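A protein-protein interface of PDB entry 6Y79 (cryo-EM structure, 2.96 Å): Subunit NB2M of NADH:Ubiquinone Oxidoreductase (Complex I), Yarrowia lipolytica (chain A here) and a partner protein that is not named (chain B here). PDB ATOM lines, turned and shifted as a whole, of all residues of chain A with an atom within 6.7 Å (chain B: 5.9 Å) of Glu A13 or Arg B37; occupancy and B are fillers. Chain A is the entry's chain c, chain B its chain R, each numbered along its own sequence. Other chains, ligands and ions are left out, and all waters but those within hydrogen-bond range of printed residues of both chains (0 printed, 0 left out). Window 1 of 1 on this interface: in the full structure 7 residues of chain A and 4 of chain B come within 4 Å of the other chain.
The guanidinium group of Arg B33 lies within salt-bridge range of the side-chain carboxylate of Glu A13, 2.7 Å away. The backbone NH of Gln B34 sits close to the side-chain hydroxyl of Tyr A17 (3.4 Å). NE of Arg B37 is in salt-bridge range of OE2 of Glu A13 (3.3 Å). The guanidinium group (NE) of Arg A16 lies close to the guanidinium group (NE) of Arg B33 (3.3 Å).
The side-chain amide oxygen (OE1) of Gln B34 sits at hydrogen-bond distance from the side-chain amide nitrogen (NE2) of Gln B38 (2.5 Å). The side-chain carboxylate (OD1) of Asp A7 is in hydrogen-bond range of the backbone NH (N) of Trp A9, 3.0 Å away.
Asp A7 touches Arg B37 (OD2 to O, 3.6 Å). OD2 of Asp A7 touches CG2 of Val B41 (3.3 Å). Pro A8 touches Val B41. CD1 of Trp A9 touches NH2 of Arg B37 (3.1 Å). Arg B33 touches Tyr A17.
Of the printed residues of chain B, Asp A7 touches Arg B37 (3.6 Å) and Val B41 (3.3 Å). Of chain B, only Arg B33 and Arg B37 come within 4 Å of Glu A13. Printed residues of chain A within 4 Å of Gln B34: Tyr A17 (3.2 Å). The nearest residue of chain A that does not touch Arg B37 is Pro A8 (5.5 Å).
Hydrophobic or aromatic side chains of chain B that line the printed part of chain A: Val B41.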
ATOM      1  N   ASP A   7     -24.113  16.100 -16.024  1.00  0.00           N
ATOM      2  CA  ASP A   7     -24.706  16.510 -17.290  1.00  0.00           C
ATOM      3  C   ASP A   7     -24.499  15.414 -18.323  1.00  0.00           C
ATOM      4  O   ASP A   7     -23.346  15.068 -18.625  1.00  0.00           O
ATOM      5  CB  ASP A   7     -24.090  17.823 -17.777  1.00  0.00           C
ATOM      6  CG  ASP A   7     -24.894  18.472 -18.894  1.00  0.00           C
ATOM      7  OD1 ASP A   7     -24.898  17.947 -20.026  1.00  0.00           O
ATOM      8  OD2 ASP A   7     -25.521  19.519 -18.644  1.00  0.00           O
ATOM      9  N   PRO A   8     -25.565  14.843 -18.892  1.00  0.00           N
ATOM     10  CA  PRO A   8     -25.371  13.765 -19.869  1.00  0.00           C
ATOM     11  C   PRO A   8     -24.796  14.219 -21.193  1.00  0.00           C
ATOM     12  O   PRO A   8     -24.097  13.443 -21.842  1.00  0.00           O
ATOM     13  CB  PRO A   8     -26.782  13.190 -20.046  1.00  0.00           C
ATOM     14  CG  PRO A   8     -27.473  13.526 -18.793  1.00  0.00           C
ATOM     15  CD  PRO A   8     -26.949  14.872 -18.402  1.00  0.00           C
ATOM     16  N   TRP A   9     -25.056  15.438 -21.644  1.00  0.00           N
ATOM     17  CA  TRP A   9     -24.411  15.950 -22.854  1.00  0.00           C
ATOM     18  C   TRP A   9     -23.263  16.853 -22.414  1.00  0.00           C
ATOM     19  O   TRP A   9     -23.277  18.070 -22.598  1.00  0.00           O
ATOM     20  CB  TRP A   9     -25.413  16.674 -23.751  1.00  0.00           C
ATOM     21  CG  TRP A   9     -26.379  15.736 -24.444  1.00  0.00           C
ATOM     22  CD1 TRP A   9     -27.649  15.446 -24.063  1.00  0.00           C
ATOM     23  CD2 TRP A   9     -26.148  14.987 -25.644  1.00  0.00           C
ATOM     24  NE1 TRP A   9     -28.228  14.569 -24.938  1.00  0.00           N
ATOM     25  CE2 TRP A   9     -27.327  14.276 -25.925  1.00  0.00           C
ATOM     26  CE3 TRP A   9     -25.061  14.847 -26.503  1.00  0.00           C
ATOM     27  CZ2 TRP A   9     -27.444  13.431 -27.025  1.00  0.00           C
ATOM     28  CZ3 TRP A   9     -25.182  14.020 -27.597  1.00  0.00           C
ATOM     29  CH2 TRP A   9     -26.364  13.323 -27.850  1.00  0.00           C
ATOM     30  N   ALA A  10     -22.239  16.234 -21.837  1.00  0.00           N
ATOM     31  CA  ALA A  10     -21.062  16.969 -21.399  1.00  0.00           C
ATOM     32  C   ALA A  10     -19.943  16.957 -22.423  1.00  0.00           C
ATOM     33  O   ALA A  10     -19.183  17.929 -22.507  1.00  0.00           O
ATOM     34  CB  ALA A  10     -20.529  16.396 -20.079  1.00  0.00           C
ATOM     35  N   ARG A  11     -19.819  15.880 -23.199  1.00  0.00           N
ATOM     36  CA  ARG A  11     -18.789  15.813 -24.219  1.00  0.00           C
ATOM     37  C   ARG A  11     -19.236  16.425 -25.533  1.00  0.00           C
ATOM     38  O   ARG A  11     -18.384  16.738 -26.372  1.00  0.00           O
ATOM     39  CB  ARG A  11     -18.367  14.359 -24.445  1.00  0.00           C
ATOM     40  CG  ARG A  11     -17.648  13.714 -23.264  1.00  0.00           C
ATOM     41  CD  ARG A  11     -17.338  12.252 -23.550  1.00  0.00           C
ATOM     42  NE  ARG A  11     -18.528  11.404 -23.499  1.00  0.00           N
ATOM     43  CZ  ARG A  11     -18.578  10.153 -23.949  1.00  0.00           C
ATOM     44  NH1 ARG A  11     -19.702   9.459 -23.860  1.00  0.00           N
ATOM     45  NH2 ARG A  11     -17.504   9.593 -24.491  1.00  0.00           N
ATOM     46  N   ARG A  12     -20.547  16.586 -25.734  1.00  0.00           N
ATOM     47  CA  ARG A  12     -21.023  17.360 -26.873  1.00  0.00           C
ATOM     48  C   ARG A  12     -20.670  18.828 -26.722  1.00  0.00           C
ATOM     49  O   ARG A  12     -19.991  19.402 -27.575  1.00  0.00           O
ATOM     50  CB  ARG A  12     -22.530  17.224 -27.047  1.00  0.00           C
ATOM     51  CG  ARG A  12     -23.023  18.061 -28.224  1.00  0.00           C
ATOM     52  CD  ARG A  12     -24.493  17.895 -28.569  1.00  0.00           C
ATOM     53  NE  ARG A  12     -24.746  18.503 -29.871  1.00  0.00           N
ATOM     54  CZ  ARG A  12     -25.944  18.682 -30.411  1.00  0.00           C
ATOM     55  NH1 ARG A  12     -27.031  18.321 -29.755  1.00  0.00           N
ATOM     56  NH2 ARG A  12     -26.055  19.243 -31.609  1.00  0.00           N
ATOM     57  N   GLU A  13     -21.112  19.451 -25.638  1.00  0.00           N
ATOM     58  CA  GLU A  13     -20.978  20.895 -25.469  1.00  0.00           C
ATOM     59  C   GLU A  13     -19.672  21.279 -24.797  1.00  0.00           C
ATOM     60  O   GLU A  13     -19.651  21.973 -23.786  1.00  0.00           O
ATOM     61  CB  GLU A  13     -22.158  21.418 -24.681  1.00  0.00           C
ATOM     62  CG  GLU A  13     -23.458  21.018 -25.282  1.00  0.00           C
ATOM     63  CD  GLU A  13     -24.583  21.380 -24.390  1.00  0.00           C
ATOM     64  OE1 GLU A  13     -24.313  21.503 -23.180  1.00  0.00           O
ATOM     65  OE2 GLU A  13     -25.708  21.547 -24.899  1.00  0.00           O
ATOM     66  N   ALA A  14     -18.566  20.819 -25.363  1.00  0.00           N
ATOM     67  CA  ALA A  14     -17.259  21.298 -24.958  1.00  0.00           C
ATOM     68  C   ALA A  14     -16.659  22.256 -25.967  1.00  0.00           C
ATOM     69  O   ALA A  14     -15.882  23.133 -25.583  1.00  0.00           O
ATOM     70  CB  ALA A  14     -16.302  20.124 -24.742  1.00  0.00           C
ATOM     71  N   TRP A  15     -17.029  22.126 -27.244  1.00  0.00           N
ATOM     72  CA  TRP A  15     -16.449  22.958 -28.289  1.00  0.00           C
ATOM     73  C   TRP A  15     -16.919  24.398 -28.224  1.00  0.00           C
ATOM     74  O   TRP A  15     -16.278  25.270 -28.814  1.00  0.00           O
ATOM     75  CB  TRP A  15     -16.768  22.385 -29.664  1.00  0.00           C
ATOM     76  CG  TRP A  15     -18.222  22.311 -30.000  1.00  0.00           C
ATOM     77  CD1 TRP A  15     -19.059  21.283 -29.740  1.00  0.00           C
ATOM     78  CD2 TRP A  15     -18.997  23.292 -30.694  1.00  0.00           C
ATOM     79  NE1 TRP A  15     -20.316  21.558 -30.206  1.00  0.00           N
ATOM     80  CE2 TRP A  15     -20.303  22.790 -30.800  1.00  0.00           C
ATOM     81  CE3 TRP A  15     -18.716  24.552 -31.227  1.00  0.00           C
ATOM     82  CZ2 TRP A  15     -21.325  23.498 -31.419  1.00  0.00           C
ATOM     83  CZ3 TRP A  15     -19.728  25.252 -31.844  1.00  0.00           C
ATOM     84  CH2 TRP A  15     -21.018  24.726 -31.933  1.00  0.00           C
ATOM     85  N   ARG A  16     -18.024  24.665 -27.530  1.00  0.00           N
ATOM     86  CA  ARG A  16     -18.493  26.032 -27.371  1.00  0.00           C
ATOM     87  C   ARG A  16     -17.662  26.816 -26.366  1.00  0.00           C
ATOM     88  O   ARG A  16     -17.775  28.042 -26.313  1.00  0.00           O
ATOM     89  CB  ARG A  16     -19.954  26.026 -26.941  1.00  0.00           C
ATOM     90  CG  ARG A  16     -20.863  25.356 -27.927  1.00  0.00           C
ATOM     91  CD  ARG A  16     -22.274  25.310 -27.411  1.00  0.00           C
ATOM     92  NE  ARG A  16     -23.210  25.054 -28.497  1.00  0.00           N
ATOM     93  CZ  ARG A  16     -23.614  23.845 -28.858  1.00  0.00           C
ATOM     94  NH1 ARG A  16     -24.464  23.705 -29.860  1.00  0.00           N
ATOM     95  NH2 ARG A  16     -23.171  22.778 -28.210  1.00  0.00           N
ATOM     96  N   TYR A  17     -16.852  26.139 -25.560  1.00  0.00           N
ATOM     97  CA  TYR A  17     -16.027  26.792 -24.557  1.00  0.00           C
ATOM     98  C   TYR A  17     -14.544  26.667 -24.842  1.00  0.00           C
ATOM     99  O   TYR A  17     -13.737  27.286 -24.144  1.00  0.00           O
ATOM    100  CB  TYR A  17     -16.342  26.214 -23.174  1.00  0.00           C
ATOM    101  CG  TYR A  17     -17.738  26.553 -22.750  1.00  0.00           C
ATOM    102  CD1 TYR A  17     -18.012  27.775 -22.162  1.00  0.00           C
ATOM    103  CD2 TYR A  17     -18.793  25.675 -22.975  1.00  0.00           C
ATOM    104  CE1 TYR A  17     -19.287  28.110 -21.784  1.00  0.00           C
ATOM    105  CE2 TYR A  17     -20.077  26.002 -22.603  1.00  0.00           C
ATOM    106  CZ  TYR A  17     -20.313  27.223 -22.006  1.00  0.00           C
ATOM    107  OH  TYR A  17     -21.578  27.582 -21.628  1.00  0.00           O
ATOM    108  N   LEU B  23     -38.524  20.466 -23.479  1.00  0.00           N
ATOM    109  CA  LEU B  23     -37.158  20.736 -23.918  1.00  0.00           C
ATOM    110  C   LEU B  23     -37.125  21.842 -24.966  1.00  0.00           C
ATOM    111  O   LEU B  23     -36.351  22.807 -24.845  1.00  0.00           O
ATOM    112  CB  LEU B  23     -36.518  19.475 -24.477  1.00  0.00           C
ATOM    113  CG  LEU B  23     -35.911  18.416 -23.556  1.00  0.00           C
ATOM    114  CD1 LEU B  23     -35.171  17.372 -24.385  1.00  0.00           C
ATOM    115  CD2 LEU B  23     -34.986  19.057 -22.545  1.00  0.00           C
ATOM    116  N   ASN B  32     -28.210  31.698 -22.784  1.00  0.00           N
ATOM    117  CA  ASN B  32     -26.919  31.085 -22.489  1.00  0.00           C
ATOM    118  C   ASN B  32     -26.949  29.589 -22.787  1.00  0.00           C
ATOM    119  O   ASN B  32     -28.005  28.960 -22.801  1.00  0.00           O
ATOM    120  CB  ASN B  32     -26.552  31.324 -21.023  1.00  0.00           C
ATOM    121  CG  ASN B  32     -25.093  31.037 -20.723  1.00  0.00           C
ATOM    122  OD1 ASN B  32     -24.307  30.735 -21.619  1.00  0.00           O
ATOM    123  ND2 ASN B  32     -24.726  31.121 -19.452  1.00  0.00           N
ATOM    124  N   ARG B  33     -25.774  29.017 -23.039  1.00  0.00           N
ATOM    125  CA  ARG B  33     -25.719  27.585 -23.297  1.00  0.00           C
ATOM    126  C   ARG B  33     -25.721  26.778 -22.004  1.00  0.00           C
ATOM    127  O   ARG B  33     -26.536  25.859 -21.853  1.00  0.00           O
ATOM    128  CB  ARG B  33     -24.495  27.238 -24.140  1.00  0.00           C
ATOM    129  CG  ARG B  33     -24.645  27.645 -25.584  1.00  0.00           C
ATOM    130  CD  ARG B  33     -25.824  26.920 -26.213  1.00  0.00           C
ATOM    131  NE  ARG B  33     -25.601  25.485 -26.334  1.00  0.00           N
ATOM    132  CZ  ARG B  33     -26.537  24.617 -26.702  1.00  0.00           C
ATOM    133  NH1 ARG B  33     -27.760  25.041 -26.982  1.00  0.00           N
ATOM    134  NH2 ARG B  33     -26.252  23.327 -26.795  1.00  0.00           N
ATOM    135  N   GLN B  34     -24.849  27.113 -21.046  1.00  0.00           N
ATOM    136  CA  GLN B  34     -24.721  26.274 -19.855  1.00  0.00           C
ATOM    137  C   GLN B  34     -25.832  26.558 -18.844  1.00  0.00           C
ATOM    138  O   GLN B  34     -26.163  25.683 -18.037  1.00  0.00           O
ATOM    139  CB  GLN B  34     -23.336  26.427 -19.208  1.00  0.00           C
ATOM    140  CG  GLN B  34     -22.966  27.784 -18.601  1.00  0.00           C
ATOM    141  CD  GLN B  34     -23.378  27.897 -17.146  1.00  0.00           C
ATOM    142  OE1 GLN B  34     -23.486  26.895 -16.443  1.00  0.00           O
ATOM    143  NE2 GLN B  34     -23.619  29.124 -16.689  1.00  0.00           N
ATOM    144  N   LEU B  35     -26.418  27.776 -18.856  1.00  0.00           N
ATOM    145  CA  LEU B  35     -27.637  27.985 -18.067  1.00  0.00           C
ATOM    146  C   LEU B  35     -28.757  27.119 -18.605  1.00  0.00           C
ATOM    147  O   LEU B  35     -29.515  26.513 -17.832  1.00  0.00           O
ATOM    148  CB  LEU B  35     -28.066  29.446 -18.065  1.00  0.00           C
ATOM    149  CG  LEU B  35     -29.097  29.941 -17.002  1.00  0.00           C
ATOM    150  CD1 LEU B  35     -28.874  31.415 -16.684  1.00  0.00           C
ATOM    151  CD2 LEU B  35     -30.625  29.689 -17.256  1.00  0.00           C
ATOM    152  N   PHE B  36     -28.850  27.024 -19.933  1.00  0.00           N
ATOM    153  CA  PHE B  36     -29.861  26.178 -20.541  1.00  0.00           C
ATOM    154  C   PHE B  36     -29.625  24.716 -20.217  1.00  0.00           C
ATOM    155  O   PHE B  36     -30.575  23.974 -19.976  1.00  0.00           O
ATOM    156  CB  PHE B  36     -29.895  26.358 -22.053  1.00  0.00           C
ATOM    157  CG  PHE B  36     -30.839  25.423 -22.718  1.00  0.00           C
ATOM    158  CD1 PHE B  36     -32.166  25.402 -22.333  1.00  0.00           C
ATOM    159  CD2 PHE B  36     -30.408  24.539 -23.687  1.00  0.00           C
ATOM    160  CE1 PHE B  36     -33.043  24.524 -22.902  1.00  0.00           C
ATOM    161  CE2 PHE B  36     -31.289  23.663 -24.275  1.00  0.00           C
ATOM    162  CZ  PHE B  36     -32.609  23.658 -23.886  1.00  0.00           C
ATOM    163  N   ARG B  37     -28.377  24.284 -20.180  1.00  0.00           N
ATOM    164  CA  ARG B  37     -28.175  22.860 -19.987  1.00  0.00           C
ATOM    165  C   ARG B  37     -28.182  22.455 -18.528  1.00  0.00           C
ATOM    166  O   ARG B  37     -28.580  21.326 -18.224  1.00  0.00           O
ATOM    167  CB  ARG B  37     -26.903  22.433 -20.694  1.00  0.00           C
ATOM    168  CG  ARG B  37     -27.062  22.696 -22.160  1.00  0.00           C
ATOM    169  CD  ARG B  37     -28.146  21.836 -22.746  1.00  0.00           C
ATOM    170  NE  ARG B  37     -27.794  20.433 -22.619  1.00  0.00           N
ATOM    171  CZ  ARG B  37     -28.637  19.432 -22.826  1.00  0.00           C
ATOM    172  NH1 ARG B  37     -29.892  19.669 -23.176  1.00  0.00           N
ATOM    173  NH2 ARG B  37     -28.221  18.191 -22.676  1.00  0.00           N
ATOM    174  N   GLN B  38     -27.806  23.363 -17.619  1.00  0.00           N
ATOM    175  CA  GLN B  38     -28.149  23.211 -16.208  1.00  0.00           C
ATOM    176  C   GLN B  38     -29.655  23.056 -16.026  1.00  0.00           C
ATOM    177  O   GLN B  38     -30.119  22.147 -15.328  1.00  0.00           O
ATOM    178  CB  GLN B  38     -27.635  24.414 -15.413  1.00  0.00           C
ATOM    179  CG  GLN B  38     -26.147  24.393 -15.085  1.00  0.00           C
ATOM    180  CD  GLN B  38     -25.678  25.703 -14.472  1.00  0.00           C
ATOM    181  OE1 GLN B  38     -26.485  26.578 -14.164  1.00  0.00           O
ATOM    182  NE2 GLN B  38     -24.368  25.851 -14.314  1.00  0.00           N
ATOM    183  N   LYS B  39     -30.436  23.908 -16.699  1.00  0.00           N
ATOM    184  CA  LYS B  39     -31.893  23.842 -16.604  1.00  0.00           C
ATOM    185  C   LYS B  39     -32.455  22.573 -17.246  1.00  0.00           C
ATOM    186  O   LYS B  39     -33.448  22.004 -16.768  1.00  0.00           O
ATOM    187  CB  LYS B  39     -32.480  25.090 -17.261  1.00  0.00           C
ATOM    188  CG  LYS B  39     -33.976  25.180 -17.228  1.00  0.00           C
ATOM    189  CD  LYS B  39     -34.455  25.389 -15.819  1.00  0.00           C
ATOM    190  CE  LYS B  39     -35.961  25.506 -15.773  1.00  0.00           C
ATOM    191  NZ  LYS B  39     -36.444  25.696 -14.382  1.00  0.00           N
ATOM    192  N   ALA B  40     -31.824  22.106 -18.322  1.00  0.00           N
ATOM    193  CA  ALA B  40     -32.292  20.910 -19.008  1.00  0.00           C
ATOM    194  C   ALA B  40     -32.025  19.663 -18.185  1.00  0.00           C
ATOM    195  O   ALA B  40     -32.890  18.785 -18.103  1.00  0.00           O
ATOM    196  CB  ALA B  40     -31.631  20.794 -20.379  1.00  0.00           C
ATOM    197  N   VAL B  41     -30.860  19.587 -17.535  1.00  0.00           N
ATOM    198  CA  VAL B  41     -30.603  18.491 -16.607  1.00  0.00           C
ATOM    199  C   VAL B  41     -31.508  18.610 -15.381  1.00  0.00           C
ATOM    200  O   VAL B  41     -31.927  17.594 -14.812  1.00  0.00           O
ATOM    201  CB  VAL B  41     -29.102  18.454 -16.251  1.00  0.00           C
ATOM    202  CG1 VAL B  41     -28.783  17.389 -15.226  1.00  0.00           C
ATOM    203  CG2 VAL B  41     -28.304  18.167 -17.492  1.00  0.00           C
ATOM    204  N   GLU B  42     -31.889  19.834 -15.003  1.00  0.00           N
ATOM    205  CA  GLU B  42     -32.798  20.008 -13.874  1.00  0.00           C
ATOM    206  C   GLU B  42     -34.191  19.451 -14.161  1.00  0.00           C
ATOM    207  O   GLU B  42     -34.769  18.748 -13.321  1.00  0.00           O
ATOM    208  CB  GLU B  42     -32.875  21.484 -13.490  1.00  0.00           C
ATOM    209  CG  GLU B  42     -33.651  21.750 -12.214  1.00  0.00           C
ATOM    210  CD  GLU B  42     -35.116  22.082 -12.467  1.00  0.00           C
ATOM    211  OE1 GLU B  42     -35.424  22.657 -13.530  1.00  0.00           O
ATOM    212  OE2 GLU B  42     -35.955  21.749 -11.612  1.00  0.00           O
